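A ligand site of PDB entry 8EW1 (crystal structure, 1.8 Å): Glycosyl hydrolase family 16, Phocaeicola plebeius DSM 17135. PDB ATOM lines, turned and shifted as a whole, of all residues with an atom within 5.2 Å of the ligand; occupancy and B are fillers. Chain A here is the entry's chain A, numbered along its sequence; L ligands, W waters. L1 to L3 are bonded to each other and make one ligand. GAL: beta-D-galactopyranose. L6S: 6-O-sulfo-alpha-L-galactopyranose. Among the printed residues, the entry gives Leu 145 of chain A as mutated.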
ATOM      1  N   ASN A  61      21.410  24.085  11.811  1.00  0.00           N
ATOM      2  CA  ASN A  61      20.166  24.709  11.367  1.00  0.00           C
ATOM      3  C   ASN A  61      20.486  25.798  10.363  1.00  0.00           C
ATOM      4  O   ASN A  61      20.922  26.893  10.753  1.00  0.00           O
ATOM      5  CB  ASN A  61      19.389  25.273  12.557  1.00  0.00           C
ATOM      6  CG  ASN A  61      17.968  25.665  12.187  1.00  0.00           C
ATOM      7  OD1 ASN A  61      17.700  26.045  11.046  1.00  0.00           O
ATOM      8  ND2 ASN A  61      17.055  25.565  13.144  1.00  0.00           N
ATOM      9  N   LYS A  63      18.690  27.874   8.940  1.00  0.00           N
ATOM     10  CA  LYS A  63      17.781  29.025   8.991  1.00  0.00           C
ATOM     11  C   LYS A  63      17.701  29.689  10.357  1.00  0.00           C
ATOM     12  O   LYS A  63      16.909  30.622  10.517  1.00  0.00           O
ATOM     13  CB  LYS A  63      16.386  28.606   8.524  1.00  0.00           C
ATOM     14  CG  LYS A  63      16.388  27.912   7.168  1.00  0.00           C
ATOM     15  CD  LYS A  63      14.985  27.728   6.604  1.00  0.00           C
ATOM     16  CE  LYS A  63      14.133  26.805   7.459  1.00  0.00           C
ATOM     17  NZ  LYS A  63      12.812  26.576   6.813  1.00  0.00           N
ATOM     18  N   TRP A  64      18.483  29.247  11.326  1.00  0.00           N
ATOM     19  CA  TRP A  64      18.438  29.812  12.674  1.00  0.00           C
ATOM     20  C   TRP A  64      19.808  29.633  13.305  1.00  0.00           C
ATOM     21  O   TRP A  64      20.252  28.498  13.492  1.00  0.00           O
ATOM     22  CB  TRP A  64      17.356  29.143  13.517  1.00  0.00           C
ATOM     23  CG  TRP A  64      17.193  29.748  14.882  1.00  0.00           C
ATOM     24  CD1 TRP A  64      17.460  31.030  15.256  1.00  0.00           C
ATOM     25  CD2 TRP A  64      16.708  29.081  16.057  1.00  0.00           C
ATOM     26  NE1 TRP A  64      17.179  31.205  16.587  1.00  0.00           N
ATOM     27  CE2 TRP A  64      16.710  30.018  17.107  1.00  0.00           C
ATOM     28  CE3 TRP A  64      16.271  27.779  16.317  1.00  0.00           C
ATOM     29  CZ2 TRP A  64      16.292  29.701  18.400  1.00  0.00           C
ATOM     30  CZ3 TRP A  64      15.855  27.462  17.600  1.00  0.00           C
ATOM     31  CH2 TRP A  64      15.870  28.419  18.622  1.00  0.00           C
ATOM     32  N   ARG A  67      19.436  30.972  19.729  1.00  0.00           N
ATOM     33  CA  ARG A  67      19.037  32.022  20.664  1.00  0.00           C
ATOM     34  C   ARG A  67      20.235  32.398  21.530  1.00  0.00           C
ATOM     35  O   ARG A  67      20.767  31.555  22.258  1.00  0.00           O
ATOM     36  CB  ARG A  67      17.871  31.552  21.522  1.00  0.00           C
ATOM     37  CG  ARG A  67      17.311  32.622  22.438  1.00  0.00           C
ATOM     38  CD  ARG A  67      16.129  32.114  23.253  1.00  0.00           C
ATOM     39  NE  ARG A  67      15.017  31.738  22.387  1.00  0.00           N
ATOM     40  CZ  ARG A  67      14.693  30.492  22.067  1.00  0.00           C
ATOM     41  NH1 ARG A  67      15.357  29.459  22.554  1.00  0.00           N
ATOM     42  NH2 ARG A  67      13.695  30.284  21.209  1.00  0.00           N
ATOM     43  N   PHE A 106      22.693  20.818  16.660  1.00  0.00           N
ATOM     44  CA  PHE A 106      21.387  20.944  16.025  1.00  0.00           C
ATOM     45  C   PHE A 106      21.374  20.120  14.734  1.00  0.00           C
ATOM     46  O   PHE A 106      22.285  20.251  13.908  1.00  0.00           O
ATOM     47  CB  PHE A 106      21.048  22.405  15.717  1.00  0.00           C
ATOM     48  CG  PHE A 106      19.578  22.692  15.620  1.00  0.00           C
ATOM     49  CD1 PHE A 106      18.760  21.915  14.810  1.00  0.00           C
ATOM     50  CD2 PHE A 106      19.009  23.708  16.353  1.00  0.00           C
ATOM     51  CE1 PHE A 106      17.404  22.162  14.726  1.00  0.00           C
ATOM     52  CE2 PHE A 106      17.654  23.969  16.279  1.00  0.00           C
ATOM     53  CZ  PHE A 106      16.851  23.189  15.460  1.00  0.00           C
ATOM     54  N   GLY A 132      15.808  19.340  23.001  1.00  0.00           N
ATOM     55  CA  GLY A 132      14.625  19.432  22.188  1.00  0.00           C
ATOM     56  C   GLY A 132      14.567  18.392  21.099  1.00  0.00           C
ATOM     57  O   GLY A 132      15.567  18.092  20.434  1.00  0.00           O
ATOM     58  N   TRP A 134      11.565  18.160  18.240  1.00  0.00           N
ATOM     59  CA  TRP A 134      10.360  18.904  17.883  1.00  0.00           C
ATOM     60  C   TRP A 134      10.202  18.995  16.366  1.00  0.00           C
ATOM     61  O   TRP A 134      11.053  18.523  15.609  1.00  0.00           O
ATOM     62  CB  TRP A 134      10.367  20.287  18.531  1.00  0.00           C
ATOM     63  CG  TRP A 134      11.649  21.067  18.379  1.00  0.00           C
ATOM     64  CD1 TRP A 134      12.871  20.764  18.920  1.00  0.00           C
ATOM     65  CD2 TRP A 134      11.829  22.308  17.685  1.00  0.00           C
ATOM     66  NE1 TRP A 134      13.793  21.718  18.578  1.00  0.00           N
ATOM     67  CE2 TRP A 134      13.176  22.684  17.823  1.00  0.00           C
ATOM     68  CE3 TRP A 134      10.978  23.132  16.939  1.00  0.00           C
ATOM     69  CZ2 TRP A 134      13.696  23.842  17.258  1.00  0.00           C
ATOM     70  CZ3 TRP A 134      11.490  24.285  16.372  1.00  0.00           C
ATOM     71  CH2 TRP A 134      12.844  24.630  16.531  1.00  0.00           C
ATOM     72  N   SER A 136       8.836  21.616  12.993  1.00  0.00           N
ATOM     73  CA  SER A 136       8.507  22.997  12.674  1.00  0.00           C
ATOM     74  C   SER A 136       8.582  23.243  11.178  1.00  0.00           C
ATOM     75  O   SER A 136       9.273  22.523  10.447  1.00  0.00           O
ATOM     76  CB  SER A 136       9.425  23.976  13.411  1.00  0.00           C
ATOM     77  OG  SER A 136      10.744  23.926  12.901  1.00  0.00           O
ATOM     78  N   ASN A 138       8.472  27.059   8.748  1.00  0.00           N
ATOM     79  CA  ASN A 138       8.206  28.463   8.468  1.00  0.00           C
ATOM     80  C   ASN A 138       8.388  28.649   6.963  1.00  0.00           C
ATOM     81  O   ASN A 138       9.514  28.744   6.474  1.00  0.00           O
ATOM     82  CB  ASN A 138       9.152  29.356   9.276  1.00  0.00           C
ATOM     83  CG  ASN A 138       8.948  30.828   9.005  1.00  0.00           C
ATOM     84  OD1 ASN A 138       8.012  31.227   8.310  1.00  0.00           O
ATOM     85  ND2 ASN A 138       9.826  31.658   9.552  1.00  0.00           N
ATOM     86  N   TRP A 143       3.681  29.479   9.407  1.00  0.00           N
ATOM     87  CA  TRP A 143       4.727  29.087  10.347  1.00  0.00           C
ATOM     88  C   TRP A 143       4.047  28.444  11.551  1.00  0.00           C
ATOM     89  O   TRP A 143       3.334  29.124  12.289  1.00  0.00           O
ATOM     90  CB  TRP A 143       5.555  30.304  10.767  1.00  0.00           C
ATOM     91  CG  TRP A 143       6.713  30.003  11.682  1.00  0.00           C
ATOM     92  CD1 TRP A 143       7.114  28.778  12.114  1.00  0.00           C
ATOM     93  CD2 TRP A 143       7.608  30.957  12.264  1.00  0.00           C
ATOM     94  NE1 TRP A 143       8.210  28.907  12.941  1.00  0.00           N
ATOM     95  CE2 TRP A 143       8.529  30.234  13.051  1.00  0.00           C
ATOM     96  CE3 TRP A 143       7.705  32.349  12.208  1.00  0.00           C
ATOM     97  CZ2 TRP A 143       9.541  30.862  13.770  1.00  0.00           C
ATOM     98  CZ3 TRP A 143       8.724  32.969  12.918  1.00  0.00           C
ATOM     99  CH2 TRP A 143       9.622  32.229  13.692  1.00  0.00           C
ATOM    100  N   LEU A 145       4.479  24.892  14.590  1.00  0.00           N
ATOM    101  CA  LEU A 145       5.465  24.167  15.374  1.00  0.00           C
ATOM    102  C   LEU A 145       4.771  23.241  16.358  1.00  0.00           C
ATOM    103  O   LEU A 145       3.817  23.647  17.030  1.00  0.00           O
ATOM    104  CB  LEU A 145       6.397  25.144  16.112  1.00  0.00           C
ATOM    105  CG  LEU A 145       7.701  24.673  16.759  1.00  0.00           C
ATOM    106  CD1 LEU A 145       8.490  25.878  17.254  1.00  0.00           C
ATOM    107  CD2 LEU A 145       7.450  23.704  17.905  1.00  0.00           C
ATOM    108  N   ASP A 147       5.897  21.193  19.645  1.00  0.00           N
ATOM    109  CA  ASP A 147       6.984  21.017  20.606  1.00  0.00           C
ATOM    110  C   ASP A 147       6.771  19.720  21.376  1.00  0.00           C
ATOM    111  O   ASP A 147       6.346  19.697  22.533  1.00  0.00           O
ATOM    112  CB  ASP A 147       7.057  22.219  21.550  1.00  0.00           C
ATOM    113  CG  ASP A 147       8.065  23.264  21.090  1.00  0.00           C
ATOM    114  OD1 ASP A 147       9.187  22.883  20.690  1.00  0.00           O
ATOM    115  OD2 ASP A 147       7.734  24.457  21.139  1.00  0.00           O
ATOM    116  N   CYS A 149       9.042  17.697  22.573  1.00  0.00           N
ATOM    117  CA  CYS A 149       9.941  17.644  23.726  1.00  0.00           C
ATOM    118  C   CYS A 149      10.773  18.913  23.744  1.00  0.00           C
ATOM    119  O   CYS A 149      11.623  19.120  22.863  1.00  0.00           O
ATOM    120  CB  CYS A 149      10.826  16.404  23.680  1.00  0.00           C
ATOM    121  SG  CYS A 149      12.113  16.375  24.940  1.00  0.00           S
ATOM    122  N   GLU A 150      10.530  19.770  24.733  1.00  0.00           N
ATOM    123  CA  GLU A 150      11.327  20.978  24.977  1.00  0.00           C
ATOM    124  C   GLU A 150      11.472  21.074  26.497  1.00  0.00           C
ATOM    125  O   GLU A 150      10.571  21.580  27.168  1.00  0.00           O
ATOM    126  CB  GLU A 150      10.656  22.210  24.393  1.00  0.00           C
ATOM    127  CG  GLU A 150      11.333  23.524  24.767  1.00  0.00           C
ATOM    128  CD  GLU A 150      10.431  24.723  24.507  1.00  0.00           C
ATOM    129  OE1 GLU A 150       9.210  24.525  24.418  1.00  0.00           O
ATOM    130  OE2 GLU A 150      10.961  25.854  24.385  1.00  0.00           O
ATOM    131  N   HIS A 167       2.488  25.634  18.582  1.00  0.00           N
ATOM    132  CA  HIS A 167       2.558  27.037  18.211  1.00  0.00           C
ATOM    133  C   HIS A 167       1.983  27.256  16.808  1.00  0.00           C
ATOM    134  O   HIS A 167       2.128  26.410  15.929  1.00  0.00           O
ATOM    135  CB  HIS A 167       4.007  27.552  18.223  1.00  0.00           C
ATOM    136  CG  HIS A 167       4.673  27.443  19.559  1.00  0.00           C
ATOM    137  ND1 HIS A 167       4.980  28.543  20.326  1.00  0.00           N
ATOM    138  CD2 HIS A 167       5.110  26.359  20.259  1.00  0.00           C
ATOM    139  CE1 HIS A 167       5.567  28.155  21.434  1.00  0.00           C
ATOM    140  NE2 HIS A 167       5.663  26.834  21.424  1.00  0.00           N
ATOM    141  N   PHE A 169       2.778  30.455  14.632  1.00  0.00           N
ATOM    142  CA  PHE A 169       3.374  31.781  14.533  1.00  0.00           C
ATOM    143  C   PHE A 169       2.639  32.621  13.488  1.00  0.00           C
ATOM    144  O   PHE A 169       2.460  33.832  13.687  1.00  0.00           O
ATOM    145  CB  PHE A 169       4.859  31.675  14.202  1.00  0.00           C
ATOM    146  CG  PHE A 169       5.697  31.222  15.358  1.00  0.00           C
ATOM    147  CD1 PHE A 169       5.905  29.873  15.583  1.00  0.00           C
ATOM    148  CD2 PHE A 169       6.257  32.140  16.232  1.00  0.00           C
ATOM    149  CE1 PHE A 169       6.672  29.450  16.650  1.00  0.00           C
ATOM    150  CE2 PHE A 169       7.017  31.725  17.299  1.00  0.00           C
ATOM    151  CZ  PHE A 169       7.227  30.376  17.514  1.00  0.00           C
ATOM    152  N   HIS A 181       1.351  35.604  17.033  1.00  0.00           N
ATOM    153  CA  HIS A 181       1.797  34.319  17.549  1.00  0.00           C
ATOM    154  C   HIS A 181       0.880  33.832  18.668  1.00  0.00           C
ATOM    155  O   HIS A 181       0.594  34.570  19.608  1.00  0.00           O
ATOM    156  CB  HIS A 181       3.238  34.427  18.045  1.00  0.00           C
ATOM    157  CG  HIS A 181       3.755  33.202  18.721  1.00  0.00           C
ATOM    158  ND1 HIS A 181       4.710  33.240  19.701  1.00  0.00           N
ATOM    159  CD2 HIS A 181       3.430  31.892  18.561  1.00  0.00           C
ATOM    160  CE1 HIS A 181       4.968  32.011  20.116  1.00  0.00           C
ATOM    161  NE2 HIS A 181       4.205  31.182  19.441  1.00  0.00           N
ATOM    162  N   ASN A 234      13.528  18.356  14.236  1.00  0.00           N
ATOM    163  CA  ASN A 234      14.656  19.058  14.810  1.00  0.00           C
ATOM    164  C   ASN A 234      15.078  18.367  16.092  1.00  0.00           C
ATOM    165  O   ASN A 234      14.223  17.991  16.898  1.00  0.00           O
ATOM    166  CB  ASN A 234      14.287  20.510  15.123  1.00  0.00           C
ATOM    167  CG  ASN A 234      13.769  21.236  13.910  1.00  0.00           C
ATOM    168  OD1 ASN A 234      14.435  21.279  12.882  1.00  0.00           O
ATOM    169  ND2 ASN A 234      12.583  21.812  14.025  1.00  0.00           N
ATOM    170  N   GLU A 238      19.630  24.161  23.256  1.00  0.00           N
ATOM    171  CA  GLU A 238      19.540  25.610  23.089  1.00  0.00           C
ATOM    172  C   GLU A 238      19.408  26.298  24.439  1.00  0.00           C
ATOM    173  O   GLU A 238      19.112  25.657  25.447  1.00  0.00           O
ATOM    174  CB  GLU A 238      18.359  25.993  22.182  1.00  0.00           C
ATOM    175  CG  GLU A 238      16.997  25.598  22.717  1.00  0.00           C
ATOM    176  CD  GLU A 238      15.875  25.895  21.735  1.00  0.00           C
ATOM    177  OE1 GLU A 238      15.909  25.336  20.618  1.00  0.00           O
ATOM    178  OE2 GLU A 238      14.974  26.688  22.070  1.00  0.00           O
HETATM  179  C1  GAL L   1       9.659  27.167  20.989  1.00  0.00           C
HETATM  180  C2  GAL L   1      10.293  28.350  20.276  1.00  0.00           C
HETATM  181  C3  GAL L   1      11.169  27.919  19.111  1.00  0.00           C
HETATM  182  C4  GAL L   1      12.092  26.809  19.566  1.00  0.00           C
HETATM  183  C5  GAL L   1      11.352  25.701  20.298  1.00  0.00           C
HETATM  184  C6  GAL L   1      12.366  24.682  20.787  1.00  0.00           C
HETATM  185  O1  GAL L   1       9.001  27.691  22.142  1.00  0.00           O
HETATM  186  O2  GAL L   1       9.268  29.213  19.783  1.00  0.00           O
HETATM  187  O3  GAL L   1      11.748  28.993  18.469  1.00  0.00           O
HETATM  188  O4  GAL L   1      13.080  27.392  20.432  1.00  0.00           O
HETATM  189  O5  GAL L   1      10.620  26.218  21.402  1.00  0.00           O
HETATM  190  O6  GAL L   1      11.728  23.496  21.267  1.00  0.00           O
HETATM  191  O1S L6S L   2      12.142  26.930  12.433  1.00  0.00           O
HETATM  192  O2S L6S L   2      13.718  25.424  13.279  1.00  0.00           O
HETATM  193  O3S L6S L   2      14.581  27.549  12.274  1.00  0.00           O
HETATM  194  C1  L6S L   2      11.186  29.692  17.352  1.00  0.00           C
HETATM  195  C2  L6S L   2      11.454  31.193  17.470  1.00  0.00           C
HETATM  196  C3  L6S L   2      12.918  31.594  17.250  1.00  0.00           C
HETATM  197  C4  L6S L   2      13.339  31.001  15.916  1.00  0.00           C
HETATM  198  C5  L6S L   2      13.104  29.497  15.943  1.00  0.00           C
HETATM  199  C6  L6S L   2      13.580  28.895  14.615  1.00  0.00           C
HETATM  200  O2  L6S L   2      10.994  31.679  18.736  1.00  0.00           O
HETATM  201  O3  L6S L   2      13.007  33.020  17.254  1.00  0.00           O
HETATM  202  O4  L6S L   2      12.700  31.512  14.815  1.00  0.00           O
HETATM  203  O5  L6S L   2      11.724  29.191  16.134  1.00  0.00           O
HETATM  204  O6  L6S L   2      13.313  27.495  14.509  1.00  0.00           O
HETATM  205  S1  L6S L   2      13.401  26.823  13.124  1.00  0.00           S
HETATM  206  C1  GAL L   3      13.774  32.108  14.060  1.00  0.00           C
HETATM  207  C2  GAL L   3      13.341  32.377  12.625  1.00  0.00           C
HETATM  208  C3  GAL L   3      14.368  33.196  11.859  1.00  0.00           C
HETATM  209  C4  GAL L   3      14.754  34.417  12.680  1.00  0.00           C
HETATM  210  C5  GAL L   3      15.251  33.968  14.047  1.00  0.00           C
HETATM  211  C6  GAL L   3      15.742  35.142  14.889  1.00  0.00           C
HETATM  212  O2  GAL L   3      13.135  31.111  11.996  1.00  0.00           O
HETATM  213  O4  GAL L   3      13.633  35.288  12.850  1.00  0.00           O
HETATM  214  O5  GAL L   3      14.184  33.311  14.711  1.00  0.00           O
HETATM  215  O6  GAL L   3      17.163  35.269  14.708  1.00  0.00           O
HETATM  216  O   HOH W   1      11.730  26.341   9.550  1.00  0.00           O
HETATM  217  O   HOH W   2      10.269  27.356  14.478  1.00  0.00           O
HETATM  218  O   HOH W   3      14.004  23.577  11.274  1.00  0.00           O
HETATM  219  O   HOH W   4       7.303  26.165  23.577  1.00  0.00           O
HETATM  220  O   HOH W   5      19.124  33.405  13.233  1.00  0.00           O
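O of Lys 63 touches C3 of GAL L3 (3.9 Å). CE3 of Trp 64 touches C6 of L6S L2, at 3.4 Å. Trp 134 touches the ligand. CH2 of Trp 143 touches O4 of L6S L2 (3.4 Å). Leu 145 touches the ligand. NE2 of His 167 touches O1 of GAL L1, at 3.5 Å. CZ of Phe 169 touches O2 of GAL L1, 3.3 Å away. Asn 234 touches the ligand. Of the 19 residues printed, 14 come within 4 Å of the ligand. Along chain A the residues within 4 Å of the ligand span positions 61 to 238.
O4 of GAL L1 sits at hydrogen-bond distance from NH2 of Arg 67 (3.1 Å). OE2 of Glu 238 sits at hydrogen-bond distance from O4 of GAL L1 (2.6 Å). ND2 of Asn 61 sits at hydrogen-bond distance from O3S of L6S L2 (3.3 Å). OD1 of Asp 147 lies within hydrogen-bond range of O6 of GAL L1, at 2.7 Å. An oxygen (O1S) of L6S L2 sits at hydrogen-bond distance from the side-chain hydroxyl (OG) of Ser 136, at 3.3 Å. The side-chain carboxylate (OE2) of Glu 150 sits at hydrogen-bond distance from an oxygen (O1) of GAL L1 (3.5 Å).
The side-chain carboxylate (OD2) of Asp 147 lies within hydrogen-bond range of a ring nitrogen (NE2) of His 167 (3.2 Å). N of Asn 234 is in hydrogen-bond range of O of Trp 134. The side-chain amide oxygen (OD1) of Asn 61 sits at hydrogen-bond distance from the backbone NH (N) of Lys 63 (3.0 Å). OE2 of Glu 238 lies within salt-bridge range of NH1 of Arg 67, 2.8 Å away. A ring nitrogen (ND1) of His 167 lies within hydrogen-bond range of a ring nitrogen (NE2) of His 181 (2.9 Å). OG of Ser 136 sits at hydrogen-bond distance from ND2 of Asn 234 (3.0 Å). The backbone NH (N) of His 167 sits at hydrogen-bond distance from the backbone carbonyl oxygen (O) of Leu 145 (2.9 Å). OD1 of Asn 61 is in hydrogen-bond range of N of Trp 64 (3.3 Å).
Water W4 lies within hydrogen-bond range of OE1 of Glu 150 (2.7 Å), O1 of GAL L1 (2.7 Å), NE2 of His 167 (2.8 Å) and OD2 of Asp 147 (3.0 Å). Water W3 lies within hydrogen-bond range of an oxygen (O2S) of L6S L2 (2.7 Å) and the side-chain amide oxygen (OD1) of Asn 234 (2.8 Å). Water W2 lies within hydrogen-bond range of an oxygen (O1S) of L6S L2 (2.8 Å) and the indole nitrogen (NE1) of Trp 143 (3.0 Å). Water W1 lies within hydrogen-bond range of the side-chain amino group (NZ) of Lys 63 (3.0 Å), an oxygen (O1S) of L6S L2 (3.0 Å) and the backbone NH (N) of Asn 138 (3.4 Å).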
